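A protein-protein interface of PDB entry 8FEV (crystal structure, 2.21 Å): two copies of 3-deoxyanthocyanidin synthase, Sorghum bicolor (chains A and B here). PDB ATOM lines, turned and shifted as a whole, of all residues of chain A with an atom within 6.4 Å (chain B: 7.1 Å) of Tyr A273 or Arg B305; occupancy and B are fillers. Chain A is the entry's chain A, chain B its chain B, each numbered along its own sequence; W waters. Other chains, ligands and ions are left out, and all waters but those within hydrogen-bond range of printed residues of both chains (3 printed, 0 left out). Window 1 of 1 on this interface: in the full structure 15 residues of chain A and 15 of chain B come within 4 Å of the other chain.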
ATOM      1  N   VAL A 201      12.754 -36.869  25.973  1.00  0.00           N
ATOM      2  CA  VAL A 201      11.658 -37.305  26.837  1.00  0.00           C
ATOM      3  C   VAL A 201      10.653 -38.092  25.988  1.00  0.00           C
ATOM      4  O   VAL A 201      11.025 -38.638  24.945  1.00  0.00           O
ATOM      5  CB  VAL A 201      11.031 -36.090  27.534  1.00  0.00           C
ATOM      6  CG1 VAL A 201      12.066 -35.460  28.466  1.00  0.00           C
ATOM      7  CG2 VAL A 201      10.519 -35.067  26.494  1.00  0.00           C
ATOM      8  N   VAL A 243       4.871 -35.286  33.556  1.00  0.00           N
ATOM      9  CA  VAL A 243       5.536 -35.978  32.470  1.00  0.00           C
ATOM     10  C   VAL A 243       6.244 -34.919  31.630  1.00  0.00           C
ATOM     11  O   VAL A 243       6.079 -33.719  31.844  1.00  0.00           O
ATOM     12  CB  VAL A 243       4.574 -36.848  31.637  1.00  0.00           C
ATOM     13  CG1 VAL A 243       3.838 -37.848  32.555  1.00  0.00           C
ATOM     14  CG2 VAL A 243       3.558 -35.995  30.858  1.00  0.00           C
ATOM     15  N   GLN A 244       7.079 -35.370  30.692  1.00  0.00           N
ATOM     16  CA  GLN A 244       7.795 -34.459  29.807  1.00  0.00           C
ATOM     17  C   GLN A 244       7.598 -34.933  28.374  1.00  0.00           C
ATOM     18  O   GLN A 244       7.687 -36.133  28.098  1.00  0.00           O
ATOM     19  CB  GLN A 244       9.286 -34.382  30.170  1.00  0.00           C
ATOM     20  CG  GLN A 244       9.551 -33.640  31.494  1.00  0.00           C
ATOM     21  CD  GLN A 244       9.988 -34.565  32.624  1.00  0.00           C
ATOM     22  OE1 GLN A 244       9.691 -35.766  32.617  1.00  0.00           O
ATOM     23  NE2 GLN A 244      10.704 -34.011  33.604  1.00  0.00           N
ATOM     24  N   LEU A 245       7.324 -33.997  27.470  1.00  0.00           N
ATOM     25  CA  LEU A 245       6.963 -34.334  26.099  1.00  0.00           C
ATOM     26  C   LEU A 245       7.745 -33.484  25.116  1.00  0.00           C
ATOM     27  O   LEU A 245       8.128 -32.350  25.411  1.00  0.00           O
ATOM     28  CB  LEU A 245       5.470 -34.121  25.835  1.00  0.00           C
ATOM     29  CG  LEU A 245       4.441 -34.661  26.819  1.00  0.00           C
ATOM     30  CD1 LEU A 245       3.100 -34.047  26.476  1.00  0.00           C
ATOM     31  CD2 LEU A 245       4.373 -36.170  26.762  1.00  0.00           C
ATOM     32  N   VAL A 246       7.952 -34.041  23.920  1.00  0.00           N
ATOM     33  CA  VAL A 246       8.581 -33.300  22.836  1.00  0.00           C
ATOM     34  C   VAL A 246       8.029 -33.825  21.514  1.00  0.00           C
ATOM     35  O   VAL A 246       7.727 -35.013  21.375  1.00  0.00           O
ATOM     36  CB  VAL A 246      10.126 -33.412  22.902  1.00  0.00           C
ATOM     37  CG1 VAL A 246      10.552 -34.835  22.574  1.00  0.00           C
ATOM     38  CG2 VAL A 246      10.787 -32.411  21.950  1.00  0.00           C
ATOM     39  N   SER A 271      13.512 -31.735  25.285  1.00  0.00           N
ATOM     40  CA  SER A 271      12.202 -31.754  25.922  1.00  0.00           C
ATOM     41  C   SER A 271      11.573 -30.379  25.724  1.00  0.00           C
ATOM     42  O   SER A 271      12.289 -29.385  25.583  1.00  0.00           O
ATOM     43  CB  SER A 271      12.340 -32.101  27.415  1.00  0.00           C
ATOM     44  OG  SER A 271      11.082 -32.102  28.065  1.00  0.00           O
ATOM     45  N   ARG A 272      10.239 -30.313  25.711  1.00  0.00           N
ATOM     46  CA  ARG A 272       9.636 -28.992  25.527  1.00  0.00           C
ATOM     47  C   ARG A 272       8.450 -28.675  26.437  1.00  0.00           C
ATOM     48  O   ARG A 272       8.354 -27.543  26.915  1.00  0.00           O
ATOM     49  CB  ARG A 272       9.199 -28.794  24.061  1.00  0.00           C
ATOM     50  CG  ARG A 272       8.804 -27.345  23.715  1.00  0.00           C
ATOM     51  CD  ARG A 272       9.801 -26.309  24.233  1.00  0.00           C
ATOM     52  NE  ARG A 272       9.340 -24.926  24.106  1.00  0.00           N
ATOM     53  CZ  ARG A 272       8.510 -24.311  24.951  1.00  0.00           C
ATOM     54  NH1 ARG A 272       7.981 -24.937  25.991  1.00  0.00           N
ATOM     55  NH2 ARG A 272       8.212 -23.027  24.754  1.00  0.00           N
ATOM     56  N   TYR A 273       7.524 -29.620  26.663  1.00  0.00           N
ATOM     57  CA  TYR A 273       6.321 -29.356  27.456  1.00  0.00           C
ATOM     58  C   TYR A 273       6.164 -30.380  28.577  1.00  0.00           C
ATOM     59  O   TYR A 273       6.269 -31.590  28.346  1.00  0.00           O
ATOM     60  CB  TYR A 273       5.032 -29.353  26.592  1.00  0.00           C
ATOM     61  CG  TYR A 273       3.875 -28.570  27.232  1.00  0.00           C
ATOM     62  CD1 TYR A 273       3.727 -27.205  27.011  1.00  0.00           C
ATOM     63  CD2 TYR A 273       2.942 -29.197  28.065  1.00  0.00           C
ATOM     64  CE1 TYR A 273       2.691 -26.473  27.597  1.00  0.00           C
ATOM     65  CE2 TYR A 273       1.896 -28.464  28.666  1.00  0.00           C
ATOM     66  CZ  TYR A 273       1.781 -27.108  28.413  1.00  0.00           C
ATOM     67  OH  TYR A 273       0.775 -26.379  28.989  1.00  0.00           O
ATOM     68  N   HIS A 274       5.848 -29.886  29.778  1.00  0.00           N
ATOM     69  CA  HIS A 274       5.874 -30.675  31.011  1.00  0.00           C
ATOM     70  C   HIS A 274       4.527 -30.628  31.738  1.00  0.00           C
ATOM     71  O   HIS A 274       4.418 -30.046  32.820  1.00  0.00           O
ATOM     72  CB  HIS A 274       6.987 -30.164  31.935  1.00  0.00           C
ATOM     73  CG  HIS A 274       8.358 -30.178  31.319  1.00  0.00           C
ATOM     74  ND1 HIS A 274       9.447 -29.588  31.926  1.00  0.00           N
ATOM     75  CD2 HIS A 274       8.813 -30.692  30.147  1.00  0.00           C
ATOM     76  CE1 HIS A 274      10.515 -29.745  31.158  1.00  0.00           C
ATOM     77  NE2 HIS A 274      10.154 -30.403  30.068  1.00  0.00           N
ATOM     78  N   PRO A 275       3.496 -31.281  31.209  1.00  0.00           N
ATOM     79  CA  PRO A 275       2.186 -31.255  31.867  1.00  0.00           C
ATOM     80  C   PRO A 275       2.076 -32.300  32.968  1.00  0.00           C
ATOM     81  O   PRO A 275       2.756 -33.322  32.960  1.00  0.00           O
ATOM     82  CB  PRO A 275       1.228 -31.613  30.725  1.00  0.00           C
ATOM     83  CG  PRO A 275       2.028 -32.628  29.955  1.00  0.00           C
ATOM     84  CD  PRO A 275       3.491 -32.198  30.059  1.00  0.00           C
ATOM     85  N   THR A 276       1.170 -32.038  33.901  1.00  0.00           N
ATOM     86  CA  THR A 276       0.619 -33.109  34.713  1.00  0.00           C
ATOM     87  C   THR A 276      -0.320 -33.968  33.871  1.00  0.00           C
ATOM     88  O   THR A 276      -0.834 -33.539  32.830  1.00  0.00           O
ATOM     89  CB  THR A 276      -0.166 -32.544  35.894  1.00  0.00           C
ATOM     90  OG1 THR A 276      -1.311 -31.832  35.392  1.00  0.00           O
ATOM     91  CG2 THR A 276       0.692 -31.602  36.720  1.00  0.00           C
ATOM     92  N   GLU A 279      -3.543 -32.179  33.450  1.00  0.00           N
ATOM     93  CA  GLU A 279      -3.530 -31.160  32.401  1.00  0.00           C
ATOM     94  C   GLU A 279      -3.618 -31.807  31.024  1.00  0.00           C
ATOM     95  O   GLU A 279      -4.423 -31.395  30.176  1.00  0.00           O
ATOM     96  CB  GLU A 279      -2.288 -30.270  32.492  1.00  0.00           C
ATOM     97  CG  GLU A 279      -2.191 -29.319  31.291  1.00  0.00           C
ATOM     98  CD  GLU A 279      -0.885 -28.578  31.221  1.00  0.00           C
ATOM     99  OE1 GLU A 279       0.010 -28.884  32.044  1.00  0.00           O
ATOM    100  OE2 GLU A 279      -0.750 -27.698  30.338  1.00  0.00           O
ATOM    101  N   LEU A 310      15.882 -27.452  30.167  1.00  0.00           N
ATOM    102  CA  LEU A 310      15.811 -27.197  28.731  1.00  0.00           C
ATOM    103  C   LEU A 310      16.879 -26.228  28.267  1.00  0.00           C
ATOM    104  O   LEU A 310      16.894 -25.853  27.091  1.00  0.00           O
ATOM    105  CB  LEU A 310      14.427 -26.641  28.329  1.00  0.00           C
ATOM    106  CG  LEU A 310      13.212 -27.270  29.012  1.00  0.00           C
ATOM    107  CD1 LEU A 310      11.935 -26.840  28.336  1.00  0.00           C
ATOM    108  CD2 LEU A 310      13.335 -28.778  29.009  1.00  0.00           C
ATOM    109  N   HIS A 322       7.296 -26.632  18.145  1.00  0.00           N
ATOM    110  CA  HIS A 322       6.064 -27.132  18.746  1.00  0.00           C
ATOM    111  C   HIS A 322       6.140 -26.795  20.228  1.00  0.00           C
ATOM    112  O   HIS A 322       6.710 -27.548  21.022  1.00  0.00           O
ATOM    113  CB  HIS A 322       5.903 -28.614  18.484  1.00  0.00           C
ATOM    114  CG  HIS A 322       5.894 -28.948  17.025  1.00  0.00           C
ATOM    115  ND1 HIS A 322       4.745 -29.322  16.353  1.00  0.00           N
ATOM    116  CD2 HIS A 322       6.884 -28.934  16.101  1.00  0.00           C
ATOM    117  CE1 HIS A 322       5.034 -29.538  15.083  1.00  0.00           C
ATOM    118  NE2 HIS A 322       6.325 -29.311  14.904  1.00  0.00           N
ATOM    119  N   ASN A 323       5.570 -25.643  20.600  1.00  0.00           N
ATOM    120  CA  ASN A 323       5.792 -25.106  21.931  1.00  0.00           C
ATOM    121  C   ASN A 323       4.604 -25.218  22.879  1.00  0.00           C
ATOM    122  O   ASN A 323       4.818 -25.248  24.094  1.00  0.00           O
ATOM    123  CB  ASN A 323       6.246 -23.652  21.820  1.00  0.00           C
ATOM    124  CG  ASN A 323       7.557 -23.536  21.059  1.00  0.00           C
ATOM    125  OD1 ASN A 323       8.610 -23.873  21.581  1.00  0.00           O
ATOM    126  ND2 ASN A 323       7.488 -23.116  19.808  1.00  0.00           N
ATOM    127  N   THR A 324       3.380 -25.313  22.369  1.00  0.00           N
ATOM    128  CA  THR A 324       2.199 -25.524  23.186  1.00  0.00           C
ATOM    129  C   THR A 324       1.879 -27.011  23.237  1.00  0.00           C
ATOM    130  O   THR A 324       2.305 -27.788  22.375  1.00  0.00           O
ATOM    131  CB  THR A 324       0.993 -24.775  22.610  1.00  0.00           C
ATOM    132  OG1 THR A 324       0.744 -25.241  21.274  1.00  0.00           O
ATOM    133  CG2 THR A 324       1.238 -23.280  22.573  1.00  0.00           C
ATOM    134  N   LEU A 325       1.067 -27.392  24.227  1.00  0.00           N
ATOM    135  CA  LEU A 325       0.600 -28.772  24.303  1.00  0.00           C
ATOM    136  C   LEU A 325      -0.127 -29.161  23.022  1.00  0.00           C
ATOM    137  O   LEU A 325       0.099 -30.240  22.449  1.00  0.00           O
ATOM    138  CB  LEU A 325      -0.302 -28.962  25.530  1.00  0.00           C
ATOM    139  CG  LEU A 325      -0.752 -30.410  25.747  1.00  0.00           C
ATOM    140  CD1 LEU A 325       0.424 -31.387  25.566  1.00  0.00           C
ATOM    141  CD2 LEU A 325      -1.406 -30.621  27.096  1.00  0.00           C
ATOM    142  N   ILE A 328       2.247 -29.768  20.242  1.00  0.00           N
ATOM    143  CA  ILE A 328       2.944 -31.047  20.362  1.00  0.00           C
ATOM    144  C   ILE A 328       2.042 -32.193  19.924  1.00  0.00           C
ATOM    145  O   ILE A 328       2.514 -33.169  19.328  1.00  0.00           O
ATOM    146  CB  ILE A 328       3.486 -31.237  21.792  1.00  0.00           C
ATOM    147  CG1 ILE A 328       4.851 -30.554  21.885  1.00  0.00           C
ATOM    148  CG2 ILE A 328       3.657 -32.724  22.099  1.00  0.00           C
ATOM    149  CD1 ILE A 328       5.213 -30.041  23.220  1.00  0.00           C
ATOM    150  N   HIS B 148      -7.321 -21.304  23.270  1.00  0.00           N
ATOM    151  CA  HIS B 148      -6.136 -22.112  23.018  1.00  0.00           C
ATOM    152  C   HIS B 148      -4.982 -21.694  23.920  1.00  0.00           C
ATOM    153  O   HIS B 148      -4.956 -20.586  24.459  1.00  0.00           O
ATOM    154  CB  HIS B 148      -5.695 -21.989  21.563  1.00  0.00           C
ATOM    155  CG  HIS B 148      -6.710 -22.491  20.602  1.00  0.00           C
ATOM    156  ND1 HIS B 148      -6.714 -23.788  20.139  1.00  0.00           N
ATOM    157  CD2 HIS B 148      -7.793 -21.886  20.059  1.00  0.00           C
ATOM    158  CE1 HIS B 148      -7.741 -23.951  19.324  1.00  0.00           C
ATOM    159  NE2 HIS B 148      -8.410 -22.814  19.261  1.00  0.00           N
ATOM    160  N   GLY B 149      -4.011 -22.599  24.061  1.00  0.00           N
ATOM    161  CA  GLY B 149      -2.776 -22.252  24.731  1.00  0.00           C
ATOM    162  C   GLY B 149      -1.905 -21.394  23.841  1.00  0.00           C
ATOM    163  O   GLY B 149      -1.970 -21.467  22.616  1.00  0.00           O
ATOM    164  N   HIS B 150      -1.080 -20.556  24.467  1.00  0.00           N
ATOM    165  CA  HIS B 150      -0.152 -19.724  23.717  1.00  0.00           C
ATOM    166  C   HIS B 150       1.141 -19.548  24.499  1.00  0.00           C
ATOM    167  O   HIS B 150       1.173 -19.674  25.724  1.00  0.00           O
ATOM    168  CB  HIS B 150      -0.753 -18.349  23.396  1.00  0.00           C
ATOM    169  CG  HIS B 150      -2.092 -18.442  22.750  1.00  0.00           C
ATOM    170  ND1 HIS B 150      -2.245 -18.608  21.391  1.00  0.00           N
ATOM    171  CD2 HIS B 150      -3.337 -18.460  23.279  1.00  0.00           C
ATOM    172  CE1 HIS B 150      -3.531 -18.711  21.107  1.00  0.00           C
ATOM    173  NE2 HIS B 150      -4.213 -18.623  22.235  1.00  0.00           N
ATOM    174  N   VAL B 151       2.207 -19.249  23.761  1.00  0.00           N
ATOM    175  CA  VAL B 151       3.504 -18.892  24.318  1.00  0.00           C
ATOM    176  C   VAL B 151       3.852 -17.518  23.777  1.00  0.00           C
ATOM    177  O   VAL B 151       4.140 -17.374  22.586  1.00  0.00           O
ATOM    178  CB  VAL B 151       4.593 -19.917  23.965  1.00  0.00           C
ATOM    179  CG1 VAL B 151       5.975 -19.425  24.430  1.00  0.00           C
ATOM    180  CG2 VAL B 151       4.255 -21.266  24.590  1.00  0.00           C
ATOM    181  N   GLN B 237      -4.304 -16.324  37.335  1.00  0.00           N
ATOM    182  CA  GLN B 237      -4.520 -17.725  36.993  1.00  0.00           C
ATOM    183  C   GLN B 237      -5.738 -17.877  36.089  1.00  0.00           C
ATOM    184  O   GLN B 237      -5.695 -18.596  35.080  1.00  0.00           O
ATOM    185  CB  GLN B 237      -4.679 -18.561  38.265  1.00  0.00           C
ATOM    186  CG  GLN B 237      -5.391 -19.888  38.027  1.00  0.00           C
ATOM    187  CD  GLN B 237      -4.568 -21.089  38.419  1.00  0.00           C
ATOM    188  OE1 GLN B 237      -3.375 -20.982  38.721  1.00  0.00           O
ATOM    189  NE2 GLN B 237      -5.208 -22.249  38.435  1.00  0.00           N
ATOM    190  N   THR B 239      -6.767 -15.849  33.970  1.00  0.00           N
ATOM    191  CA  THR B 239      -6.402 -15.363  32.647  1.00  0.00           C
ATOM    192  C   THR B 239      -5.430 -16.295  31.933  1.00  0.00           C
ATOM    193  O   THR B 239      -5.625 -16.626  30.760  1.00  0.00           O
ATOM    194  CB  THR B 239      -5.796 -13.973  32.780  1.00  0.00           C
ATOM    195  OG1 THR B 239      -6.733 -13.135  33.454  1.00  0.00           O
ATOM    196  CG2 THR B 239      -5.499 -13.375  31.420  1.00  0.00           C
ATOM    197  N   SER B 240      -4.367 -16.726  32.613  1.00  0.00           N
ATOM    198  CA  SER B 240      -3.275 -17.404  31.929  1.00  0.00           C
ATOM    199  C   SER B 240      -3.175 -18.895  32.221  1.00  0.00           C
ATOM    200  O   SER B 240      -2.380 -19.583  31.565  1.00  0.00           O
ATOM    201  CB  SER B 240      -1.948 -16.711  32.267  1.00  0.00           C
ATOM    202  OG  SER B 240      -2.008 -15.364  31.820  1.00  0.00           O
ATOM    203  N   GLY B 241      -3.965 -19.418  33.154  1.00  0.00           N
ATOM    204  CA  GLY B 241      -3.895 -20.825  33.480  1.00  0.00           C
ATOM    205  C   GLY B 241      -2.844 -21.160  34.503  1.00  0.00           C
ATOM    206  O   GLY B 241      -2.676 -22.337  34.834  1.00  0.00           O
ATOM    207  N   GLU B 242      -2.157 -20.152  35.035  1.00  0.00           N
ATOM    208  CA  GLU B 242      -1.018 -20.324  35.927  1.00  0.00           C
ATOM    209  C   GLU B 242      -0.552 -18.935  36.348  1.00  0.00           C
ATOM    210  O   GLU B 242      -1.130 -17.935  35.910  1.00  0.00           O
ATOM    211  CB  GLU B 242       0.100 -21.082  35.204  1.00  0.00           C
ATOM    212  CG  GLU B 242       0.641 -20.274  34.000  1.00  0.00           C
ATOM    213  CD  GLU B 242       1.689 -21.007  33.141  1.00  0.00           C
ATOM    214  OE1 GLU B 242       1.701 -22.269  33.081  1.00  0.00           O
ATOM    215  OE2 GLU B 242       2.521 -20.290  32.531  1.00  0.00           O
ATOM    216  N   HIS B 274       6.553 -21.319  36.779  1.00  0.00           N
ATOM    217  CA  HIS B 274       5.168 -21.051  36.376  1.00  0.00           C
ATOM    218  C   HIS B 274       4.227 -22.080  36.996  1.00  0.00           C
ATOM    219  O   HIS B 274       3.774 -23.014  36.314  1.00  0.00           O
ATOM    220  CB  HIS B 274       5.030 -21.063  34.856  1.00  0.00           C
ATOM    221  CG  HIS B 274       6.006 -20.168  34.161  1.00  0.00           C
ATOM    222  ND1 HIS B 274       6.058 -20.036  32.790  1.00  0.00           N
ATOM    223  CD2 HIS B 274       6.975 -19.360  34.653  1.00  0.00           C
ATOM    224  CE1 HIS B 274       7.020 -19.188  32.468  1.00  0.00           C
ATOM    225  NE2 HIS B 274       7.595 -18.766  33.582  1.00  0.00           N
ATOM    226  N   PRO B 275       3.876 -21.922  38.267  1.00  0.00           N
ATOM    227  CA  PRO B 275       2.986 -22.883  38.911  1.00  0.00           C
ATOM    228  C   PRO B 275       1.523 -22.496  38.755  1.00  0.00           C
ATOM    229  O   PRO B 275       1.171 -21.329  38.578  1.00  0.00           O
ATOM    230  CB  PRO B 275       3.410 -22.780  40.377  1.00  0.00           C
ATOM    231  CG  PRO B 275       3.689 -21.297  40.533  1.00  0.00           C
ATOM    232  CD  PRO B 275       4.247 -20.832  39.190  1.00  0.00           C
ATOM    233  N   THR B 276       0.664 -23.506  38.838  1.00  0.00           N
ATOM    234  CA  THR B 276      -0.726 -23.227  39.170  1.00  0.00           C
ATOM    235  C   THR B 276      -0.845 -22.831  40.642  1.00  0.00           C
ATOM    236  O   THR B 276       0.034 -23.117  41.470  1.00  0.00           O
ATOM    237  CB  THR B 276      -1.601 -24.439  38.938  1.00  0.00           C
ATOM    238  OG1 THR B 276      -1.224 -25.440  39.887  1.00  0.00           O
ATOM    239  CG2 THR B 276      -1.452 -24.973  37.520  1.00  0.00           C
ATOM    240  N   GLU B 301     -10.218 -25.857  37.642  1.00  0.00           N
ATOM    241  CA  GLU B 301     -10.187 -26.554  36.370  1.00  0.00           C
ATOM    242  C   GLU B 301      -8.916 -26.189  35.619  1.00  0.00           C
ATOM    243  O   GLU B 301      -8.450 -25.046  35.662  1.00  0.00           O
ATOM    244  CB  GLU B 301     -11.409 -26.175  35.526  1.00  0.00           C
ATOM    245  CG  GLU B 301     -11.470 -24.669  35.240  1.00  0.00           C
ATOM    246  CD  GLU B 301     -12.807 -24.192  34.690  1.00  0.00           C
ATOM    247  OE1 GLU B 301     -13.555 -23.541  35.455  1.00  0.00           O
ATOM    248  OE2 GLU B 301     -13.099 -24.449  33.498  1.00  0.00           O
ATOM    249  N   GLU B 302      -8.367 -27.166  34.920  1.00  0.00           N
ATOM    250  CA  GLU B 302      -7.229 -26.937  34.048  1.00  0.00           C
ATOM    251  C   GLU B 302      -7.651 -26.056  32.881  1.00  0.00           C
ATOM    252  O   GLU B 302      -8.569 -26.407  32.133  1.00  0.00           O
ATOM    253  CB  GLU B 302      -6.692 -28.281  33.564  1.00  0.00           C
ATOM    254  CG  GLU B 302      -6.035 -29.092  34.681  1.00  0.00           C
ATOM    255  CD  GLU B 302      -4.680 -28.528  35.072  1.00  0.00           C
ATOM    256  OE1 GLU B 302      -4.014 -27.923  34.201  1.00  0.00           O
ATOM    257  OE2 GLU B 302      -4.276 -28.689  36.244  1.00  0.00           O
ATOM    258  N   ARG B 303      -7.009 -24.904  32.742  1.00  0.00           N
ATOM    259  CA  ARG B 303      -7.273 -24.004  31.631  1.00  0.00           C
ATOM    260  C   ARG B 303      -6.128 -24.034  30.633  1.00  0.00           C
ATOM    261  O   ARG B 303      -5.015 -24.461  30.952  1.00  0.00           O
ATOM    262  CB  ARG B 303      -7.456 -22.556  32.114  1.00  0.00           C
ATOM    263  CG  ARG B 303      -8.276 -22.361  33.356  1.00  0.00           C
ATOM    264  CD  ARG B 303      -8.305 -20.878  33.753  1.00  0.00           C
ATOM    265  NE  ARG B 303      -9.644 -20.505  34.190  1.00  0.00           N
ATOM    266  CZ  ARG B 303     -10.136 -20.807  35.385  1.00  0.00           C
ATOM    267  NH1 ARG B 303      -9.405 -21.433  36.293  1.00  0.00           N
ATOM    268  NH2 ARG B 303     -11.393 -20.476  35.675  1.00  0.00           N
ATOM    269  N   PRO B 304      -6.365 -23.557  29.414  1.00  0.00           N
ATOM    270  CA  PRO B 304      -5.256 -23.350  28.476  1.00  0.00           C
ATOM    271  C   PRO B 304      -4.169 -22.498  29.116  1.00  0.00           C
ATOM    272  O   PRO B 304      -4.444 -21.486  29.767  1.00  0.00           O
ATOM    273  CB  PRO B 304      -5.909 -22.612  27.301  1.00  0.00           C
ATOM    274  CG  PRO B 304      -7.372 -22.809  27.465  1.00  0.00           C
ATOM    275  CD  PRO B 304      -7.631 -22.987  28.926  1.00  0.00           C
ATOM    276  N   ARG B 305      -2.923 -22.903  28.913  1.00  0.00           N
ATOM    277  CA  ARG B 305      -1.809 -22.136  29.441  1.00  0.00           C
ATOM    278  C   ARG B 305      -1.438 -21.046  28.449  1.00  0.00           C
ATOM    279  O   ARG B 305      -1.129 -21.336  27.284  1.00  0.00           O
ATOM    280  CB  ARG B 305      -0.614 -23.044  29.725  1.00  0.00           C
ATOM    281  CG  ARG B 305      -0.980 -24.195  30.634  1.00  0.00           C
ATOM    282  CD  ARG B 305      -1.306 -23.700  32.018  1.00  0.00           C
ATOM    283  NE  ARG B 305      -0.999 -24.701  33.039  1.00  0.00           N
ATOM    284  CZ  ARG B 305      -1.814 -25.692  33.387  1.00  0.00           C
ATOM    285  NH1 ARG B 305      -3.000 -25.854  32.811  1.00  0.00           N
ATOM    286  NH2 ARG B 305      -1.433 -26.542  34.338  1.00  0.00           N
ATOM    287  N   VAL B 306      -1.486 -19.800  28.907  1.00  0.00           N
ATOM    288  CA  VAL B 306      -0.961 -18.665  28.168  1.00  0.00           C
ATOM    289  C   VAL B 306       0.260 -18.194  28.945  1.00  0.00           C
ATOM    290  O   VAL B 306       0.143 -17.530  29.985  1.00  0.00           O
ATOM    291  CB  VAL B 306      -1.998 -17.547  27.997  1.00  0.00           C
ATOM    292  CG1 VAL B 306      -1.413 -16.465  27.160  1.00  0.00           C
ATOM    293  CG2 VAL B 306      -3.275 -18.094  27.334  1.00  0.00           C
ATOM    294  N   THR B 307       1.439 -18.532  28.445  1.00  0.00           N
ATOM    295  CA  THR B 307       2.650 -18.459  29.238  1.00  0.00           C
ATOM    296  C   THR B 307       3.672 -17.530  28.583  1.00  0.00           C
ATOM    297  O   THR B 307       3.633 -17.271  27.377  1.00  0.00           O
ATOM    298  CB  THR B 307       3.215 -19.897  29.486  1.00  0.00           C
ATOM    299  OG1 THR B 307       4.434 -19.814  30.223  1.00  0.00           O
ATOM    300  CG2 THR B 307       3.485 -20.637  28.192  1.00  0.00           C
HETATM  301  O   HOH W   1       0.276 -29.131  34.454  1.00  0.00           O
HETATM  302  O   HOH W   2      -1.534 -29.145  36.378  1.00  0.00           O
HETATM  303  O   HOH W   3      -2.225 -23.980  21.161  1.00  0.00           O
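OE1 of Glu A279 lies within salt-bridge range of NH2 of Arg B305.
The side-chain hydroxyl of Tyr A273 sits at hydrogen-bond distance from the side-chain carboxylate of Glu A279, 2.4 Å away.
The guanidinium group (NH1) of Arg B305 sits at hydrogen-bond distance from the backbone carbonyl oxygen (O) of Arg B303.
O of His B150 is in hydrogen-bond range of N of Thr B307, 3.0 Å away.
N of His B150 lies within hydrogen-bond range of O of Arg B305.
The backbone carbonyl oxygen (O) of Gly B241 sits at hydrogen-bond distance from the guanidinium group (NE) of Arg B305 (3.4 Å).
NE2 of His B150 lies close to O of His B148 (3.1 Å).
CG of Arg B305 touches OH of Tyr A273, at 3.2 Å.
Glu B302 touches Glu A279 (OE1 to CB, 3.4 Å).
CG2 of Thr A324 touches O of Gly B149, at 3.7 Å.
Thr A324 touches His B150.
Of chain B, only Arg B305 (3.2 Å) comes within 4 Å of Tyr A273.
Of the printed residues of chain B, Glu A279 touches Glu B302 (3.4 Å) and Arg B305 (3.5 Å).
Of the printed residues of chain B, Thr A324 touches Gly B149 and His B150.
Of the printed residues of chain A, Gly B149 touches Thr A324.
Printed residues of chain A within 4 Å of His B150: Thr A324.
Thr B276 touches none of the printed residues of chain A.
Printed residues of chain A within 4 Å of Glu B302: Glu A279.
Of chain A, only Tyr A273 (3.2 Å) and Glu A279 (3.5 Å) come within 4 Å of Arg B305.
The nearest residue of chain B that does not touch Tyr A273 is Glu B242 (5.9 Å).
The nearest residue of chain A that does not touch Arg B305 is Thr A276 (5.4 Å).
The nearest printed residue of chain A that does not touch His B150 is Asn A323 (6.8 Å).
Of the 18 printed residues of chain A, 3 touch a printed residue of chain B.
Printed residues of chain A that touch a printed residue of chain B: Tyr A273, Glu A279 and Thr A324.
Hydrophobic or aromatic side chains of chain A within 4 Å of the printed part of chain B: Tyr A273.
Along chain A the printed residues that touch a printed residue of chain B span positions 273 to 324.
Among the printed residues, Asp or Glu carboxylates within 4 Å of a Lys or Arg side-chain nitrogen of the other chain: Glu A279 with Arg B305.
3 positions are printed for both chains.
Water W1 lies within hydrogen-bond range of OE1 of Glu A279 (2.4 Å), N of Thr A276 (3.1 Å) and NH2 of Arg B305 (3.1 Å).
Water W2 lies within hydrogen-bond range of OE2 of Glu B302, OG1 of Thr A276 and NH2 of Arg B305.
Water W3 bridges O of Gly B149 and OG1 of Thr A324.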
